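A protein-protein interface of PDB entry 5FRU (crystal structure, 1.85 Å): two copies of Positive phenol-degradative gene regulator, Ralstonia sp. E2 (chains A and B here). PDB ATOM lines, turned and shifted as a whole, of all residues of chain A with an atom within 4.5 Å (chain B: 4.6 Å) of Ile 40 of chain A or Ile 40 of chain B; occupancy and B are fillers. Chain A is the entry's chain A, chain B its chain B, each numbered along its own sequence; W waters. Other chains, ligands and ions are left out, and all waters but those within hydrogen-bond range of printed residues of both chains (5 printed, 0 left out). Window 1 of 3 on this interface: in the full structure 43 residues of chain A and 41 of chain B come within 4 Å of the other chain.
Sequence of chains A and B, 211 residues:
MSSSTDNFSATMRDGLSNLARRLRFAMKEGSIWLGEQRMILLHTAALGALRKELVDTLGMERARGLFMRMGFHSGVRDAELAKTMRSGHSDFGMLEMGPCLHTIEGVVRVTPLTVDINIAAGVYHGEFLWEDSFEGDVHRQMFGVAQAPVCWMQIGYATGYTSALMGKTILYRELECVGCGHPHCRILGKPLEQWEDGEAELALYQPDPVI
The guanidinium group (NH2) of Arg 38 of chain B sits at hydrogen-bond distance from the backbone carbonyl oxygen (O) of Gly 106 of chain A (3.3 Å). The backbone carbonyl oxygen (O) of Val 107 of chain A is in hydrogen-bond range of the guanidinium group (NH2) of Arg 38 of chain B (3.4 Å). O of Glu 105 of chain A sits at hydrogen-bond distance from N of Leu 41 of chain B, 2.9 Å away. The backbone NH (N) of Leu 42 of chain B is in hydrogen-bond range of the backbone carbonyl oxygen (O) of Ile 40 of chain A (2.9 Å). The backbone carbonyl oxygen of Leu 42 of chain A is in hydrogen-bond range of the backbone NH of Ile 40 of chain B (2.9 Å). The backbone NH (N) of Leu 41 of chain A sits at hydrogen-bond distance from the backbone carbonyl oxygen (O) of Glu 105 of chain B (2.8 Å). The backbone carbonyl oxygen of Ile 40 of chain A sits close to the backbone carbonyl oxygen of Ile 40 of chain B, at 3.4 Å. The backbone NH (N) of Thr 44 of chain A sits at hydrogen-bond distance from the backbone carbonyl oxygen (O) of Arg 38 of chain B.
Printed residues of chain B within 4 Å of Ile 40 of chain A: Ile 40 (3.4 Å), Leu 41 (3.4 Å), Leu 42 (2.9 Å), Thr 44 (3.96 Å), Leu 47 (3.7 Å), Glu 105 (3.4 Å) and Gly 106 (3.6 Å). Printed residues of chain A within 4 Å of Met 39 of chain B: Leu 41 and Leu 42. Of the printed residues of chain B, Leu 41 of chain A touches Met 39 (3.9 Å), Ile 40 (3.4 Å), Leu 41 (3.5 Å) and Glu 105 (2.8 Å). Of the printed residues of chain A, Leu 41 of chain B touches Met 39, Ile 40, Leu 41 and Glu 105. The nearest printed residue of chain B that does not touch Ile 40 of chain A is Phe 134 of chain B (4.01 Å). The nearest residue of chain A that does not touch Ile 40 of chain B is Val 107 of chain A (4.1 Å).
Printed residues of chain B that touch a printed residue of chain A: Arg 38, Met 39, Ile 40, Leu 41, Leu 42, Thr 44, Leu 47, Glu 105 and Gly 106. Of the 10 printed residues of chain A, 10 touch a printed residue of chain B. Hydrophobic or aromatic side chains of chain A that line the printed part of chain B: Met 39, Ile 40, Leu 41, Leu 47 and Phe 134.
Water W2 lies within hydrogen-bond range of the backbone carbonyl oxygen of Gly 106 of chain A, the backbone carbonyl oxygen of Met 39 of chain B and the guanidinium group of Arg 38 of chain B. Water W5 bridges O of Met 39 of chain A (2.6 Å) and O of Gly 106 of chain B (2.6 Å). Water W3 bridges the backbone carbonyl oxygen (O) of Leu 41 of chain A and the side-chain carboxylate (OE1) of Glu 105 of chain B. Water W4 bridges the side-chain carboxylate (OE1) of Glu 105 of chain A (2.7 Å) and the backbone carbonyl oxygen (O) of Leu 41 of chain B (2.9 Å). Water W1 lies within hydrogen-bond range of O of Arg 38 of chain B (2.9 Å) and N of Thr 44 of chain A (3.1 Å).
Among the printed residues, pairs that only touch across the chains: Met 39 of chain A with Leu 42 of chain B (3.3 Å), Glu 105 of chain A with Ile 40 of chain B (3.4 Å), Ile 40 of chain A with Glu 105 of chain B (3.4 Å), Leu 42 of chain A with Met 39 of chain B (3.4 Å), Leu 41 of chain A with Ile 40 of chain B (3.4 Å), Ile 40 of chain A with Leu 41 of chain B (3.4 Å), Leu 41 of chain A with Leu 41 of chain B (3.5 Å), Phe 134 of chain A with Arg 38 of chain B (3.5 Å), Gly 106 of chain A with Ile 40 of chain B (3.6 Å), Leu 47 of chain A with Ile 40 of chain B (3.6 Å), Ile 40 of chain A with Gly 106 of chain B (3.6 Å), Ile 40 of chain A with Leu 47 of chain B (3.7 Å), Met 39 of chain A with Leu 41 of chain B (3.8 Å), Leu 41 of chain A with Met 39 of chain B (3.9 Å), Phe 134 of chain A with Ile 40 of chain B (3.9 Å) and Ile 40 of chain A with Thr 44 of chain B (3.96 Å).
The backbone NH (N) of Phe 134 of chain A is in hydrogen-bond range of the backbone carbonyl oxygen (O) of Val 107 of chain A (2.9 Å).
Ile 40 of chain B touches its own counterpart, Ile 40 of chain A. Ile 40 of chain A touches Leu 41 of chain B, and with the chains exchanged Leu 41 of chain A touches Ile 40 of chain B. Ile 40 of chain A touches Leu 42 of chain B, and with the chains exchanged Leu 42 of chain A touches Ile 40 of chain B. Leu 41 of chain A touches Glu 105 of chain B, and with the chains exchanged Glu 105 of chain A touches Leu 41 of chain B. Positions printed for both chains: 39, 40, 41, 42, 44, 47, 105, 106, 107 and 134. Of the 24 pairs that touch across the chains among the printed residues, 18 have their exchanged pair printed and touching as well.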
ATOM      1  N   MET A  39      24.367   2.222  13.988  1.00  0.00           N
ATOM      2  CA  MET A  39      24.779   1.151  13.074  1.00  0.00           C
ATOM      3  C   MET A  39      23.582   0.259  12.767  1.00  0.00           C
ATOM      4  O   MET A  39      22.688   0.130  13.599  1.00  0.00           O
ATOM      5  CB  MET A  39      25.894   0.270  13.681  1.00  0.00           C
ATOM      6  CG  MET A  39      27.048   1.029  14.370  1.00  0.00           C
ATOM      7  SD  MET A  39      28.015   1.986  13.203  1.00  0.00           S
ATOM      8  CE  MET A  39      28.937   0.665  12.390  1.00  0.00           C
ATOM      9  N   ILE A  40      23.573  -0.378  11.595  1.00  0.00           N
ATOM     10  CA  ILE A  40      22.679  -1.513  11.361  1.00  0.00           C
ATOM     11  C   ILE A  40      23.496  -2.746  10.962  1.00  0.00           C
ATOM     12  O   ILE A  40      24.622  -2.631  10.469  1.00  0.00           O
ATOM     13  CB  ILE A  40      21.638  -1.238  10.250  1.00  0.00           C
ATOM     14  CG1 ILE A  40      22.334  -0.935   8.918  1.00  0.00           C
ATOM     15  CG2 ILE A  40      20.706  -0.112  10.668  1.00  0.00           C
ATOM     16  CD1 ILE A  40      21.459  -1.192   7.676  1.00  0.00           C
ATOM     17  N   LEU A  41      22.921  -3.923  11.171  1.00  0.00           N
ATOM     18  CA  LEU A  41      23.482  -5.144  10.605  1.00  0.00           C
ATOM     19  C   LEU A  41      22.835  -5.368   9.246  1.00  0.00           C
ATOM     20  O   LEU A  41      21.619  -5.466   9.140  1.00  0.00           O
ATOM     21  CB  LEU A  41      23.243  -6.340  11.524  1.00  0.00           C
ATOM     22  CG  LEU A  41      24.145  -6.435  12.748  1.00  0.00           C
ATOM     23  CD1 LEU A  41      23.519  -7.363  13.797  1.00  0.00           C
ATOM     24  CD2 LEU A  41      25.520  -6.928  12.337  1.00  0.00           C
ATOM     25  N   LEU A  42      23.652  -5.449   8.211  1.00  0.00           N
ATOM     26  CA  LEU A  42      23.158  -5.517   6.849  1.00  0.00           C
ATOM     27  C   LEU A  42      23.721  -6.767   6.219  1.00  0.00           C
ATOM     28  O   LEU A  42      24.917  -7.031   6.354  1.00  0.00           O
ATOM     29  CB  LEU A  42      23.577  -4.280   6.044  1.00  0.00           C
ATOM     30  CG  LEU A  42      22.978  -4.169   4.639  1.00  0.00           C
ATOM     31  CD1 LEU A  42      21.466  -4.308   4.701  1.00  0.00           C
ATOM     32  CD2 LEU A  42      23.361  -2.854   3.997  1.00  0.00           C
ATOM     33  N   THR A  44      25.354  -9.168   3.592  1.00  0.00           N
ATOM     34  CA  THR A  44      26.267  -8.899   2.491  1.00  0.00           C
ATOM     35  C   THR A  44      25.564  -9.182   1.159  1.00  0.00           C
ATOM     36  O   THR A  44      25.865  -8.545   0.151  1.00  0.00           O
ATOM     37  CB  THR A  44      27.561  -9.721   2.612  1.00  0.00           C
ATOM     38  OG1 THR A  44      27.235 -11.111   2.694  1.00  0.00           O
ATOM     39  CG2 THR A  44      28.340  -9.304   3.863  1.00  0.00           C
ATOM     40  N   LEU A  47      23.821  -5.989   0.020  1.00  0.00           N
ATOM     41  CA  LEU A  47      24.807  -5.071  -0.540  1.00  0.00           C
ATOM     42  C   LEU A  47      25.225  -5.556  -1.923  1.00  0.00           C
ATOM     43  O   LEU A  47      25.469  -4.768  -2.837  1.00  0.00           O
ATOM     44  CB  LEU A  47      26.015  -4.968   0.384  1.00  0.00           C
ATOM     45  CG  LEU A  47      25.897  -3.868   1.434  1.00  0.00           C
ATOM     46  CD1 LEU A  47      27.181  -3.789   2.239  1.00  0.00           C
ATOM     47  CD2 LEU A  47      25.568  -2.510   0.785  1.00  0.00           C
ATOM     48  N   GLU A 105      33.503  -4.796  12.758  1.00  0.00           N
ATOM     49  CA  GLU A 105      32.319  -4.539  11.934  1.00  0.00           C
ATOM     50  C   GLU A 105      32.046  -5.677  10.944  1.00  0.00           C
ATOM     51  O   GLU A 105      31.080  -5.624  10.157  1.00  0.00           O
ATOM     52  CB  GLU A 105      32.487  -3.205  11.201  1.00  0.00           C
ATOM     53  CG  GLU A 105      32.289  -2.036  12.144  1.00  0.00           C
ATOM     54  CD  GLU A 105      32.987  -0.774  11.700  1.00  0.00           C
ATOM     55  OE1 GLU A 105      33.294  -0.610  10.498  1.00  0.00           O
ATOM     56  OE2 GLU A 105      33.221   0.068  12.578  1.00  0.00           O
ATOM     57  N   GLY A 106      32.892  -6.708  10.995  1.00  0.00           N
ATOM     58  CA  GLY A 106      32.736  -7.898  10.170  1.00  0.00           C
ATOM     59  C   GLY A 106      33.125  -7.732   8.715  1.00  0.00           C
ATOM     60  O   GLY A 106      32.700  -8.514   7.854  1.00  0.00           O
ATOM     61  N   VAL A 107      33.931  -6.720   8.424  1.00  0.00           N
ATOM     62  CA  VAL A 107      34.213  -6.361   7.045  1.00  0.00           C
ATOM     63  C   VAL A 107      35.367  -7.186   6.484  1.00  0.00           C
ATOM     64  O   VAL A 107      35.302  -7.687   5.367  1.00  0.00           O
ATOM     65  CB  VAL A 107      34.522  -4.851   6.931  1.00  0.00           C
ATOM     66  CG1 VAL A 107      35.140  -4.528   5.589  1.00  0.00           C
ATOM     67  CG2 VAL A 107      33.226  -4.044   7.170  1.00  0.00           C
ATOM     68  N   PHE A 134      34.842  -9.066   2.897  1.00  0.00           N
ATOM     69  CA  PHE A 134      33.447  -9.353   2.551  1.00  0.00           C
ATOM     70  C   PHE A 134      33.169  -8.880   1.125  1.00  0.00           C
ATOM     71  O   PHE A 134      32.444  -9.523   0.366  1.00  0.00           O
ATOM     72  CB  PHE A 134      32.472  -8.700   3.538  1.00  0.00           C
ATOM     73  CG  PHE A 134      31.951  -7.371   3.084  1.00  0.00           C
ATOM     74  CD1 PHE A 134      32.667  -6.215   3.337  1.00  0.00           C
ATOM     75  CD2 PHE A 134      30.742  -7.277   2.404  1.00  0.00           C
ATOM     76  CE1 PHE A 134      32.194  -4.977   2.920  1.00  0.00           C
ATOM     77  CE2 PHE A 134      30.263  -6.049   1.980  1.00  0.00           C
ATOM     78  CZ  PHE A 134      30.985  -4.899   2.243  1.00  0.00           C
ATOM     79  N   ARG B  38      26.249 -13.999   5.975  1.00  0.00           N
ATOM     80  CA  ARG B  38      27.288 -13.086   6.418  1.00  0.00           C
ATOM     81  C   ARG B  38      26.719 -11.660   6.478  1.00  0.00           C
ATOM     82  O   ARG B  38      26.044 -11.225   5.549  1.00  0.00           O
ATOM     83  CB  ARG B  38      28.505 -13.140   5.502  1.00  0.00           C
ATOM     84  CG  ARG B  38      29.712 -12.502   6.135  1.00  0.00           C
ATOM     85  CD  ARG B  38      30.932 -12.510   5.212  1.00  0.00           C
ATOM     86  NE  ARG B  38      31.981 -11.690   5.796  1.00  0.00           N
ATOM     87  CZ  ARG B  38      33.229 -11.626   5.353  1.00  0.00           C
ATOM     88  NH1 ARG B  38      33.621 -12.372   4.319  1.00  0.00           N
ATOM     89  NH2 ARG B  38      34.090 -10.833   5.970  1.00  0.00           N
ATOM     90  N   MET B  39      27.008 -10.967   7.579  1.00  0.00           N
ATOM     91  CA  MET B  39      26.514  -9.617   7.869  1.00  0.00           C
ATOM     92  C   MET B  39      27.676  -8.646   8.043  1.00  0.00           C
ATOM     93  O   MET B  39      28.767  -9.068   8.415  1.00  0.00           O
ATOM     94  CB  MET B  39      25.680  -9.621   9.160  1.00  0.00           C
ATOM     95  CG  MET B  39      24.690 -10.783   9.290  1.00  0.00           C
ATOM     96  SD  MET B  39      23.372 -10.631   8.093  1.00  0.00           S
ATOM     97  CE  MET B  39      22.445  -9.261   8.757  1.00  0.00           C
ATOM     98  N   ILE B  40      27.456  -7.356   7.779  1.00  0.00           N
ATOM     99  CA  ILE B  40      28.373  -6.334   8.304  1.00  0.00           C
ATOM    100  C   ILE B  40      27.640  -5.288   9.156  1.00  0.00           C
ATOM    101  O   ILE B  40      26.454  -5.022   8.958  1.00  0.00           O
ATOM    102  CB  ILE B  40      29.145  -5.590   7.188  1.00  0.00           C
ATOM    103  CG1 ILE B  40      28.174  -4.896   6.234  1.00  0.00           C
ATOM    104  CG2 ILE B  40      30.081  -6.558   6.440  1.00  0.00           C
ATOM    105  CD1 ILE B  40      28.840  -3.780   5.397  1.00  0.00           C
ATOM    106  N   LEU B  41      28.357  -4.738  10.127  1.00  0.00           N
ATOM    107  CA  LEU B  41      27.929  -3.540  10.840  1.00  0.00           C
ATOM    108  C   LEU B  41      28.251  -2.321  10.005  1.00  0.00           C
ATOM    109  O   LEU B  41      29.420  -2.032   9.764  1.00  0.00           O
ATOM    110  CB  LEU B  41      28.630  -3.419  12.188  1.00  0.00           C
ATOM    111  CG  LEU B  41      28.039  -4.256  13.321  1.00  0.00           C
ATOM    112  CD1 LEU B  41      28.880  -4.066  14.574  1.00  0.00           C
ATOM    113  CD2 LEU B  41      26.593  -3.845  13.570  1.00  0.00           C
ATOM    114  N   LEU B  42      27.224  -1.609   9.565  1.00  0.00           N
ATOM    115  CA  LEU B  42      27.418  -0.453   8.696  1.00  0.00           C
ATOM    116  C   LEU B  42      26.832   0.796   9.348  1.00  0.00           C
ATOM    117  O   LEU B  42      25.738   0.758   9.901  1.00  0.00           O
ATOM    118  CB  LEU B  42      26.775  -0.710   7.323  1.00  0.00           C
ATOM    119  CG  LEU B  42      26.873   0.375   6.244  1.00  0.00           C
ATOM    120  CD1 LEU B  42      28.315   0.756   5.981  1.00  0.00           C
ATOM    121  CD2 LEU B  42      26.201  -0.099   4.948  1.00  0.00           C
ATOM    122  N   THR B  44      24.867   4.067   9.858  1.00  0.00           N
ATOM    123  CA  THR B  44      23.679   4.591   9.171  1.00  0.00           C
ATOM    124  C   THR B  44      24.034   5.856   8.395  1.00  0.00           C
ATOM    125  O   THR B  44      23.435   6.152   7.354  1.00  0.00           O
ATOM    126  CB  THR B  44      22.520   4.888  10.140  1.00  0.00           C
ATOM    127  OG1 THR B  44      22.934   5.868  11.104  1.00  0.00           O
ATOM    128  CG2 THR B  44      22.069   3.597  10.838  1.00  0.00           C
ATOM    129  N   LEU B  47      25.219   4.704   4.936  1.00  0.00           N
ATOM    130  CA  LEU B  47      24.048   4.387   4.123  1.00  0.00           C
ATOM    131  C   LEU B  47      23.315   5.665   3.677  1.00  0.00           C
ATOM    132  O   LEU B  47      22.854   5.767   2.529  1.00  0.00           O
ATOM    133  CB  LEU B  47      23.083   3.477   4.896  1.00  0.00           C
ATOM    134  CG  LEU B  47      23.008   2.013   4.449  1.00  0.00           C
ATOM    135  CD1 LEU B  47      21.782   1.344   5.035  1.00  0.00           C
ATOM    136  CD2 LEU B  47      22.991   1.896   2.944  1.00  0.00           C
ATOM    137  N   GLU B 105      18.685  -6.562  14.078  1.00  0.00           N
ATOM    138  CA  GLU B 105      19.572  -5.952  13.084  1.00  0.00           C
ATOM    139  C   GLU B 105      19.721  -4.444  13.281  1.00  0.00           C
ATOM    140  O   GLU B 105      20.494  -3.788  12.568  1.00  0.00           O
ATOM    141  CB  GLU B 105      19.066  -6.275  11.671  1.00  0.00           C
ATOM    142  CG  GLU B 105      19.457  -7.701  11.277  1.00  0.00           C
ATOM    143  CD  GLU B 105      18.568  -8.329  10.223  1.00  0.00           C
ATOM    144  OE1 GLU B 105      17.900  -7.614   9.445  1.00  0.00           O
ATOM    145  OE2 GLU B 105      18.551  -9.568  10.174  1.00  0.00           O
ATOM    146  N   GLY B 106      18.978  -3.908  14.245  1.00  0.00           N
ATOM    147  CA  GLY B 106      19.044  -2.491  14.567  1.00  0.00           C
ATOM    148  C   GLY B 106      18.370  -1.592  13.551  1.00  0.00           C
ATOM    149  O   GLY B 106      18.583  -0.378  13.537  1.00  0.00           O
ATOM    150  N   VAL B 107      17.530  -2.182  12.716  1.00  0.00           N
ATOM    151  CA  VAL B 107      16.896  -1.449  11.628  1.00  0.00           C
ATOM    152  C   VAL B 107      15.691  -0.650  12.136  1.00  0.00           C
ATOM    153  O   VAL B 107      15.492   0.519  11.783  1.00  0.00           O
ATOM    154  CB  VAL B 107      16.475  -2.427  10.498  1.00  0.00           C
ATOM    155  CG1 VAL B 107      15.584  -1.735   9.479  1.00  0.00           C
ATOM    156  CG2 VAL B 107      17.707  -3.018   9.825  1.00  0.00           C
ATOM    157  N   PHE B 134      15.304   3.410  11.283  1.00  0.00           N
ATOM    158  CA  PHE B 134      16.525   4.123  10.999  1.00  0.00           C
ATOM    159  C   PHE B 134      16.368   4.846   9.673  1.00  0.00           C
ATOM    160  O   PHE B 134      16.933   5.895   9.471  1.00  0.00           O
ATOM    161  CB  PHE B 134      17.740   3.200  10.961  1.00  0.00           C
ATOM    162  CG  PHE B 134      18.083   2.719   9.580  1.00  0.00           C
ATOM    163  CD1 PHE B 134      17.437   1.620   9.039  1.00  0.00           C
ATOM    164  CD2 PHE B 134      19.031   3.380   8.821  1.00  0.00           C
ATOM    165  CE1 PHE B 134      17.745   1.186   7.770  1.00  0.00           C
ATOM    166  CE2 PHE B 134      19.347   2.946   7.553  1.00  0.00           C
ATOM    167  CZ  PHE B 134      18.704   1.869   7.026  1.00  0.00           C
HETATM  168  O   HOH W   1      24.241 -12.042   3.484  1.00  0.00           O
HETATM  169  O   HOH W   2      30.956 -10.384   8.057  1.00  0.00           O
HETATM  170  O   HOH W   3      19.365  -5.703   7.917  1.00  0.00           O
HETATM  171  O   HOH W   4      31.621  -0.744   8.421  1.00  0.00           O
HETATM  172  O   HOH W   5      20.526   0.775  14.823  1.00  0.00           O
